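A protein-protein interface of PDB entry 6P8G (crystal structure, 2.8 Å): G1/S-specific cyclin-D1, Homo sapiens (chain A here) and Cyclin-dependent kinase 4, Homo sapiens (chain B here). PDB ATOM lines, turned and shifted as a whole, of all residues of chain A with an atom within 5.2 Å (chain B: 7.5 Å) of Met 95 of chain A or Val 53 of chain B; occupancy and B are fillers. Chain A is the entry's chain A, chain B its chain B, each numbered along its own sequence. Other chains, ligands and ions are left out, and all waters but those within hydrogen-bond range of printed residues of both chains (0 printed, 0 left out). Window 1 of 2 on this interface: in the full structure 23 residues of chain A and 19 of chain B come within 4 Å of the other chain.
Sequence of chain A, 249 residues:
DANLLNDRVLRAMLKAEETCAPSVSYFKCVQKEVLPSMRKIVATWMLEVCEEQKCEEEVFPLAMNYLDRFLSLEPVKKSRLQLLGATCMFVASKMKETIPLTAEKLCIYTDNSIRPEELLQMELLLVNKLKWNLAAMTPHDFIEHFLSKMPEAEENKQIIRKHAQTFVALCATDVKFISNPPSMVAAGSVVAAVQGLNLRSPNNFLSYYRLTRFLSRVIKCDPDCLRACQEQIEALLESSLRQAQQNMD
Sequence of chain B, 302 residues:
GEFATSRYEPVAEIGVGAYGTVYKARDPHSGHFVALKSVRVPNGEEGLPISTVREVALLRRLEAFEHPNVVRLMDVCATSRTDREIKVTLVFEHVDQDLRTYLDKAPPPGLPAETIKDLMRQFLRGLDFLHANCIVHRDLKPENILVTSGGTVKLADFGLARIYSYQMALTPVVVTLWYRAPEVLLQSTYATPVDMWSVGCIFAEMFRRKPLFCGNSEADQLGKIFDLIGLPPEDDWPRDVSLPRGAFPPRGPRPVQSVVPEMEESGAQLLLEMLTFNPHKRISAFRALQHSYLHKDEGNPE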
ATOM      1  N   LEU A  62      14.673  13.059 -18.648  1.00  0.00           N
ATOM      2  CA  LEU A  62      14.344  13.602 -19.962  1.00  0.00           C
ATOM      3  C   LEU A  62      13.994  12.490 -20.942  1.00  0.00           C
ATOM      4  O   LEU A  62      13.102  12.652 -21.782  1.00  0.00           O
ATOM      5  CB  LEU A  62      15.506  14.440 -20.491  1.00  0.00           C
ATOM      6  CG  LEU A  62      15.297  15.111 -21.848  1.00  0.00           C
ATOM      7  CD1 LEU A  62      14.065  16.002 -21.815  1.00  0.00           C
ATOM      8  CD2 LEU A  62      16.529  15.907 -22.253  1.00  0.00           C
ATOM      9  N   TYR A  66      10.541  11.783 -23.089  1.00  0.00           N
ATOM     10  CA  TYR A  66      10.415  11.419 -24.496  1.00  0.00           C
ATOM     11  C   TYR A  66       9.611  10.135 -24.661  1.00  0.00           C
ATOM     12  O   TYR A  66       8.829  10.003 -25.609  1.00  0.00           O
ATOM     13  CB  TYR A  66      11.798  11.260 -25.128  1.00  0.00           C
ATOM     14  CG  TYR A  66      12.629  12.524 -25.164  1.00  0.00           C
ATOM     15  CD1 TYR A  66      12.030  13.777 -25.127  1.00  0.00           C
ATOM     16  CD2 TYR A  66      14.015  12.464 -25.240  1.00  0.00           C
ATOM     17  CE1 TYR A  66      12.787  14.932 -25.161  1.00  0.00           C
ATOM     18  CE2 TYR A  66      14.781  13.615 -25.275  1.00  0.00           C
ATOM     19  CZ  TYR A  66      14.161  14.845 -25.235  1.00  0.00           C
ATOM     20  OH  TYR A  66      14.919  15.993 -25.271  1.00  0.00           O
ATOM     21  N   VAL A  91      18.710  10.336 -27.590  1.00  0.00           N
ATOM     22  CA  VAL A  91      18.441  11.737 -27.899  1.00  0.00           C
ATOM     23  C   VAL A  91      18.675  12.615 -26.676  1.00  0.00           C
ATOM     24  O   VAL A  91      19.240  13.709 -26.784  1.00  0.00           O
ATOM     25  CB  VAL A  91      17.009  11.894 -28.445  1.00  0.00           C
ATOM     26  CG1 VAL A  91      16.675  13.364 -28.649  1.00  0.00           C
ATOM     27  CG2 VAL A  91      16.846  11.120 -29.746  1.00  0.00           C
ATOM     28  N   ALA A  92      18.249  12.153 -25.498  1.00  0.00           N
ATOM     29  CA  ALA A  92      18.426  12.946 -24.285  1.00  0.00           C
ATOM     30  C   ALA A  92      19.901  13.152 -23.974  1.00  0.00           C
ATOM     31  O   ALA A  92      20.301  14.230 -23.518  1.00  0.00           O
ATOM     32  CB  ALA A  92      17.718  12.276 -23.107  1.00  0.00           C
ATOM     33  N   SER A  93      20.725  12.129 -24.216  1.00  0.00           N
ATOM     34  CA  SER A  93      22.159  12.269 -23.995  1.00  0.00           C
ATOM     35  C   SER A  93      22.763  13.320 -24.916  1.00  0.00           C
ATOM     36  O   SER A  93      23.708  14.015 -24.530  1.00  0.00           O
ATOM     37  CB  SER A  93      22.853  10.921 -24.190  1.00  0.00           C
ATOM     38  OG  SER A  93      24.191  10.960 -23.724  1.00  0.00           O
ATOM     39  N   LYS A  94      22.230  13.453 -26.134  1.00  0.00           N
ATOM     40  CA  LYS A  94      22.712  14.493 -27.036  1.00  0.00           C
ATOM     41  C   LYS A  94      22.308  15.881 -26.559  1.00  0.00           C
ATOM     42  O   LYS A  94      23.011  16.859 -26.836  1.00  0.00           O
ATOM     43  CB  LYS A  94      22.187  14.248 -28.449  1.00  0.00           C
ATOM     44  CG  LYS A  94      22.761  13.021 -29.133  1.00  0.00           C
ATOM     45  CD  LYS A  94      22.172  12.852 -30.522  1.00  0.00           C
ATOM     46  CE  LYS A  94      22.816  11.695 -31.261  1.00  0.00           C
ATOM     47  NZ  LYS A  94      22.281  11.559 -32.647  1.00  0.00           N
ATOM     48  N   MET A  95      21.190  15.986 -25.840  1.00  0.00           N
ATOM     49  CA  MET A  95      20.678  17.274 -25.396  1.00  0.00           C
ATOM     50  C   MET A  95      21.286  17.751 -24.086  1.00  0.00           C
ATOM     51  O   MET A  95      21.203  18.948 -23.784  1.00  0.00           O
ATOM     52  CB  MET A  95      19.154  17.207 -25.237  1.00  0.00           C
ATOM     53  CG  MET A  95      18.396  16.980 -26.532  1.00  0.00           C
ATOM     54  SD  MET A  95      18.240  18.481 -27.518  1.00  0.00           S
ATOM     55  CE  MET A  95      17.478  19.587 -26.335  1.00  0.00           C
ATOM     56  N   LYS A  96      21.895  16.858 -23.303  1.00  0.00           N
ATOM     57  CA  LYS A  96      22.334  17.203 -21.959  1.00  0.00           C
ATOM     58  C   LYS A  96      23.773  16.824 -21.633  1.00  0.00           C
ATOM     59  O   LYS A  96      24.255  17.206 -20.560  1.00  0.00           O
ATOM     60  CB  LYS A  96      21.415  16.549 -20.915  1.00  0.00           C
ATOM     61  CG  LYS A  96      19.998  17.101 -20.901  1.00  0.00           C
ATOM     62  CD  LYS A  96      19.998  18.607 -20.703  1.00  0.00           C
ATOM     63  CE  LYS A  96      18.598  19.132 -20.436  1.00  0.00           C
ATOM     64  NZ  LYS A  96      18.598  20.604 -20.208  1.00  0.00           N
ATOM     65  N   GLU A  97      24.472  16.100 -22.503  1.00  0.00           N
ATOM     66  CA  GLU A  97      25.813  15.622 -22.206  1.00  0.00           C
ATOM     67  C   GLU A  97      26.811  16.157 -23.223  1.00  0.00           C
ATOM     68  O   GLU A  97      26.481  16.368 -24.394  1.00  0.00           O
ATOM     69  CB  GLU A  97      25.863  14.088 -22.184  1.00  0.00           C
ATOM     70  CG  GLU A  97      25.071  13.468 -21.045  1.00  0.00           C
ATOM     71  CD  GLU A  97      25.582  12.097 -20.655  1.00  0.00           C
ATOM     72  OE1 GLU A  97      25.228  11.111 -21.336  1.00  0.00           O
ATOM     73  OE2 GLU A  97      26.340  12.005 -19.668  1.00  0.00           O
ATOM     74  N   GLU A 123      15.636   7.029 -34.101  1.00  0.00           N
ATOM     75  CA  GLU A 123      15.894   8.407 -33.697  1.00  0.00           C
ATOM     76  C   GLU A 123      15.139   9.383 -34.587  1.00  0.00           C
ATOM     77  O   GLU A 123      14.477  10.305 -34.097  1.00  0.00           O
ATOM     78  CB  GLU A 123      17.395   8.697 -33.730  1.00  0.00           C
ATOM     79  CG  GLU A 123      17.746  10.142 -33.404  1.00  0.00           C
ATOM     80  CD  GLU A 123      19.156  10.514 -33.817  1.00  0.00           C
ATOM     81  OE1 GLU A 123      19.921  10.993 -32.953  1.00  0.00           O
ATOM     82  OE2 GLU A 123      19.498  10.330 -35.004  1.00  0.00           O
ATOM     83  N   TRP A 132      10.460  17.704 -33.092  1.00  0.00           N
ATOM     84  CA  TRP A 132      11.704  18.320 -32.640  1.00  0.00           C
ATOM     85  C   TRP A 132      11.529  19.133 -31.361  1.00  0.00           C
ATOM     86  O   TRP A 132      12.348  20.007 -31.062  1.00  0.00           O
ATOM     87  CB  TRP A 132      12.322  19.185 -33.744  1.00  0.00           C
ATOM     88  CG  TRP A 132      12.757  18.382 -34.928  1.00  0.00           C
ATOM     89  CD1 TRP A 132      11.952  17.792 -35.859  1.00  0.00           C
ATOM     90  CD2 TRP A 132      14.103  18.069 -35.305  1.00  0.00           C
ATOM     91  NE1 TRP A 132      12.713  17.133 -36.793  1.00  0.00           N
ATOM     92  CE2 TRP A 132      14.037  17.288 -36.475  1.00  0.00           C
ATOM     93  CE3 TRP A 132      15.356  18.369 -34.763  1.00  0.00           C
ATOM     94  CZ2 TRP A 132      15.177  16.807 -37.116  1.00  0.00           C
ATOM     95  CZ3 TRP A 132      16.485  17.893 -35.402  1.00  0.00           C
ATOM     96  CH2 TRP A 132      16.388  17.120 -36.565  1.00  0.00           C
ATOM     97  N   LEU A 134      12.362  18.850 -28.289  1.00  0.00           N
ATOM     98  CA  LEU A 134      13.249  18.112 -27.402  1.00  0.00           C
ATOM     99  C   LEU A 134      13.720  18.923 -26.204  1.00  0.00           C
ATOM    100  O   LEU A 134      14.198  18.333 -25.229  1.00  0.00           O
ATOM    101  CB  LEU A 134      14.470  17.609 -28.182  1.00  0.00           C
ATOM    102  CG  LEU A 134      14.155  16.985 -29.543  1.00  0.00           C
ATOM    103  CD1 LEU A 134      15.430  16.579 -30.266  1.00  0.00           C
ATOM    104  CD2 LEU A 134      13.222  15.795 -29.381  1.00  0.00           C
ATOM    105  N   ALA A 135      13.596  20.248 -26.248  1.00  0.00           N
ATOM    106  CA  ALA A 135      14.048  21.106 -25.154  1.00  0.00           C
ATOM    107  C   ALA A 135      12.952  21.250 -24.096  1.00  0.00           C
ATOM    108  O   ALA A 135      12.501  22.345 -23.756  1.00  0.00           O
ATOM    109  CB  ALA A 135      14.485  22.463 -25.693  1.00  0.00           C
ATOM    110  N   GLY B  47      23.781   8.996 -35.738  1.00  0.00           N
ATOM    111  CA  GLY B  47      22.540   9.692 -36.001  1.00  0.00           C
ATOM    112  C   GLY B  47      22.752  11.175 -36.251  1.00  0.00           C
ATOM    113  O   GLY B  47      23.749  11.604 -36.842  1.00  0.00           O
ATOM    114  N   LEU B  48      21.794  11.973 -35.782  1.00  0.00           N
ATOM    115  CA  LEU B  48      21.832  13.406 -36.013  1.00  0.00           C
ATOM    116  C   LEU B  48      22.943  14.055 -35.188  1.00  0.00           C
ATOM    117  O   LEU B  48      23.247  13.608 -34.079  1.00  0.00           O
ATOM    118  CB  LEU B  48      20.489  14.037 -35.663  1.00  0.00           C
ATOM    119  CG  LEU B  48      19.271  13.475 -36.396  1.00  0.00           C
ATOM    120  CD1 LEU B  48      18.035  13.554 -35.515  1.00  0.00           C
ATOM    121  CD2 LEU B  48      19.046  14.214 -37.706  1.00  0.00           C
ATOM    122  N   PRO B  49      23.569  15.109 -35.712  1.00  0.00           N
ATOM    123  CA  PRO B  49      24.626  15.789 -34.958  1.00  0.00           C
ATOM    124  C   PRO B  49      24.083  16.432 -33.691  1.00  0.00           C
ATOM    125  O   PRO B  49      22.893  16.730 -33.569  1.00  0.00           O
ATOM    126  CB  PRO B  49      25.144  16.849 -35.942  1.00  0.00           C
ATOM    127  CG  PRO B  49      24.686  16.385 -37.290  1.00  0.00           C
ATOM    128  CD  PRO B  49      23.388  15.685 -37.054  1.00  0.00           C
ATOM    129  N   ILE B  50      24.988  16.642 -32.732  1.00  0.00           N
ATOM    130  CA  ILE B  50      24.601  17.269 -31.471  1.00  0.00           C
ATOM    131  C   ILE B  50      24.112  18.689 -31.712  1.00  0.00           C
ATOM    132  O   ILE B  50      23.094  19.115 -31.153  1.00  0.00           O
ATOM    133  CB  ILE B  50      25.774  17.240 -30.474  1.00  0.00           C
ATOM    134  CG1 ILE B  50      26.314  15.820 -30.320  1.00  0.00           C
ATOM    135  CG2 ILE B  50      25.342  17.796 -29.127  1.00  0.00           C
ATOM    136  CD1 ILE B  50      27.635  15.755 -29.589  1.00  0.00           C
ATOM    137  N   SER B  51      24.825  19.445 -32.551  1.00  0.00           N
ATOM    138  CA  SER B  51      24.430  20.822 -32.823  1.00  0.00           C
ATOM    139  C   SER B  51      23.088  20.895 -33.541  1.00  0.00           C
ATOM    140  O   SER B  51      22.348  21.869 -33.368  1.00  0.00           O
ATOM    141  CB  SER B  51      25.509  21.525 -33.649  1.00  0.00           C
ATOM    142  OG  SER B  51      26.618  21.880 -32.841  1.00  0.00           O
ATOM    143  N   THR B  52      22.753  19.880 -34.339  1.00  0.00           N
ATOM    144  CA  THR B  52      21.502  19.920 -35.090  1.00  0.00           C
ATOM    145  C   THR B  52      20.300  19.742 -34.172  1.00  0.00           C
ATOM    146  O   THR B  52      19.329  20.503 -34.252  1.00  0.00           O
ATOM    147  CB  THR B  52      21.511  18.849 -36.182  1.00  0.00           C
ATOM    148  OG1 THR B  52      22.608  19.083 -37.073  1.00  0.00           O
ATOM    149  CG2 THR B  52      20.209  18.885 -36.970  1.00  0.00           C
ATOM    150  N   VAL B  53      20.348  18.745 -33.284  1.00  0.00           N
ATOM    151  CA  VAL B  53      19.185  18.457 -32.448  1.00  0.00           C
ATOM    152  C   VAL B  53      18.981  19.538 -31.395  1.00  0.00           C
ATOM    153  O   VAL B  53      17.852  19.765 -30.945  1.00  0.00           O
ATOM    154  CB  VAL B  53      19.317  17.066 -31.800  1.00  0.00           C
ATOM    155  CG1 VAL B  53      19.230  15.978 -32.856  1.00  0.00           C
ATOM    156  CG2 VAL B  53      20.616  16.958 -31.018  1.00  0.00           C
ATOM    157  N   ARG B  54      20.050  20.224 -30.985  1.00  0.00           N
ATOM    158  CA  ARG B  54      19.927  21.192 -29.900  1.00  0.00           C
ATOM    159  C   ARG B  54      19.444  22.549 -30.403  1.00  0.00           C
ATOM    160  O   ARG B  54      18.590  23.178 -29.768  1.00  0.00           O
ATOM    161  CB  ARG B  54      21.261  21.331 -29.164  1.00  0.00           C
ATOM    162  CG  ARG B  54      21.718  20.052 -28.472  1.00  0.00           C
ATOM    163  CD  ARG B  54      22.277  20.321 -27.081  1.00  0.00           C
ATOM    164  NE  ARG B  54      23.707  20.614 -27.107  1.00  0.00           N
ATOM    165  CZ  ARG B  54      24.630  19.902 -26.467  1.00  0.00           C
ATOM    166  NH1 ARG B  54      24.276  18.844 -25.752  1.00  0.00           N
ATOM    167  NH2 ARG B  54      25.909  20.246 -26.547  1.00  0.00           N
ATOM    168  N   GLU B  55      19.973  23.016 -31.535  1.00  0.00           N
ATOM    169  CA  GLU B  55      19.578  24.328 -32.041  1.00  0.00           C
ATOM    170  C   GLU B  55      18.151  24.313 -32.576  1.00  0.00           C
ATOM    171  O   GLU B  55      17.412  25.291 -32.413  1.00  0.00           O
ATOM    172  CB  GLU B  55      20.555  24.793 -33.120  1.00  0.00           C
ATOM    173  CG  GLU B  55      21.991  24.922 -32.639  1.00  0.00           C
ATOM    174  CD  GLU B  55      22.982  25.039 -33.781  1.00  0.00           C
ATOM    175  OE1 GLU B  55      24.085  25.582 -33.560  1.00  0.00           O
ATOM    176  OE2 GLU B  55      22.660  24.589 -34.901  1.00  0.00           O
ATOM    177  N   VAL B  56      17.744  23.215 -33.216  1.00  0.00           N
ATOM    178  CA  VAL B  56      16.384  23.130 -33.741  1.00  0.00           C
ATOM    179  C   VAL B  56      15.381  22.979 -32.603  1.00  0.00           C
ATOM    180  O   VAL B  56      14.274  23.527 -32.659  1.00  0.00           O
ATOM    181  CB  VAL B  56      16.274  21.979 -34.758  1.00  0.00           C
ATOM    182  CG1 VAL B  56      14.841  21.832 -35.249  1.00  0.00           C
ATOM    183  CG2 VAL B  56      17.209  22.221 -35.932  1.00  0.00           C
ATOM    184  N   ALA B  57      15.752  22.244 -31.551  1.00  0.00           N
ATOM    185  CA  ALA B  57      14.860  22.103 -30.405  1.00  0.00           C
ATOM    186  C   ALA B  57      14.685  23.429 -29.676  1.00  0.00           C
ATOM    187  O   ALA B  57      13.587  23.743 -29.202  1.00  0.00           O
ATOM    188  CB  ALA B  57      15.391  21.035 -29.451  1.00  0.00           C
ATOM    189  N   LEU B  58      15.757  24.218 -29.577  1.00  0.00           N
ATOM    190  CA  LEU B  58      15.648  25.529 -28.946  1.00  0.00           C
ATOM    191  C   LEU B  58      14.789  26.467 -29.784  1.00  0.00           C
ATOM    192  O   LEU B  58      14.020  27.267 -29.239  1.00  0.00           O
ATOM    193  CB  LEU B  58      17.041  26.116 -28.714  1.00  0.00           C
ATOM    194  CG  LEU B  58      17.182  27.636 -28.644  1.00  0.00           C
ATOM    195  CD1 LEU B  58      16.566  28.181 -27.359  1.00  0.00           C
ATOM    196  CD2 LEU B  58      18.646  28.027 -28.749  1.00  0.00           C
ATOM    197  N   LEU B  59      14.900  26.379 -31.113  1.00  0.00           N
ATOM    198  CA  LEU B  59      13.993  27.133 -31.971  1.00  0.00           C
ATOM    199  C   LEU B  59      12.556  26.664 -31.785  1.00  0.00           C
ATOM    200  O   LEU B  59      11.621  27.472 -31.817  1.00  0.00           O
ATOM    201  CB  LEU B  59      14.419  27.001 -33.434  1.00  0.00           C
ATOM    202  CG  LEU B  59      15.565  27.902 -33.899  1.00  0.00           C
ATOM    203  CD1 LEU B  59      15.669  27.899 -35.415  1.00  0.00           C
ATOM    204  CD2 LEU B  59      15.391  29.319 -33.375  1.00  0.00           C
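Hydrophobic or aromatic side chains of chain B within 4 Å of the printed part of chain A: Leu 48, Ile 50, Val 56 and Ala 57.
Along chain B the printed residues that touch a printed residue of chain A span positions 47 to 57.
Printed residues of chain A that touch a printed residue of chain B: Lys 94, Met 95, Lys 96, Glu 97, Glu 123, Trp 132, Leu 134 and Ala 135.
Among the printed residues, 14 pairs touch across the chains.
Among the printed residues, merely in contact across the chains: Lys 94 of chain A with Gly 47 of chain B, Lys 94 of chain A with Ile 50 of chain B, Met 95 of chain A with Arg 54 of chain B, Lys 96 of chain A with Arg 54 of chain B, Glu 97 of chain A with Arg 54 of chain B, Glu 123 of chain A with Gly 47 of chain B, Trp 132 of chain A with Val 56 of chain B, Trp 132 of chain A with Ala 57 of chain B, Leu 134 of chain A with Ala 57 of chain B and Ala 135 of chain A with Ala 57 of chain B.
Met 95 of chain A touches two residues of chain B.
Val 53 of chain B touches just one residue of chain A: Met 95.
Of the printed residues of chain B, Ala 135 of chain A touches Ala 57 (3.8 Å).
Printed residues of chain B within 4 Å of Glu 97 of chain A: Arg 54.
Of the printed residues of chain A, Arg 54 of chain B touches Lys 94 (2.6 Å), Met 95 (3.6 Å), Lys 96 (3.95 Å) and Glu 97 (3.6 Å).
Of the printed residues of chain B, Lys 94 of chain A touches Gly 47 (3.7 Å), Leu 48 (2.7 Å), Ile 50 (3.4 Å) and Arg 54 (2.6 Å).
Pro 49 of chain B touches none of the printed residues of chain A.
The nearest residue of chain B that does not touch Met 95 of chain A is Ala 57 of chain B (4.02 Å).
The nearest printed residue of chain A that does not touch Val 53 of chain B is Trp 132 of chain A (4.04 Å).
The nearest printed residue of chain B that does not touch Leu 134 of chain A is Val 53 of chain B (4.1 Å).
The side-chain amino group (NZ) of Lys 94 of chain A is in hydrogen-bond range of the backbone carbonyl oxygen (O) of Leu 48 of chain B.
NH1 of Arg 54 of chain B sits at hydrogen-bond distance from O of Lys 94 of chain A, 2.6 Å away.
N of Leu 48 of chain B sits at hydrogen-bond distance from OE2 of Glu 123 of chain A (2.9 Å).
The backbone carbonyl oxygen (O) of Val 53 of chain B lies close to the side-chain sulfur (SD) of Met 95 of chain A, at 3.7 Å.
OH of Tyr 66 of chain A is in hydrogen-bond range of O of Leu 134 of chain A, at 2.4 Å.
The side-chain hydroxyl (OG) of Ser 93 of chain A is in hydrogen-bond range of the side-chain carboxylate (OE1) of Glu 97 of chain A (2.6 Å).
The side-chain amino group of Lys 94 of chain A lies within salt-bridge range of the side-chain carboxylate of Glu 123 of chain A, 2.4 Å away.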
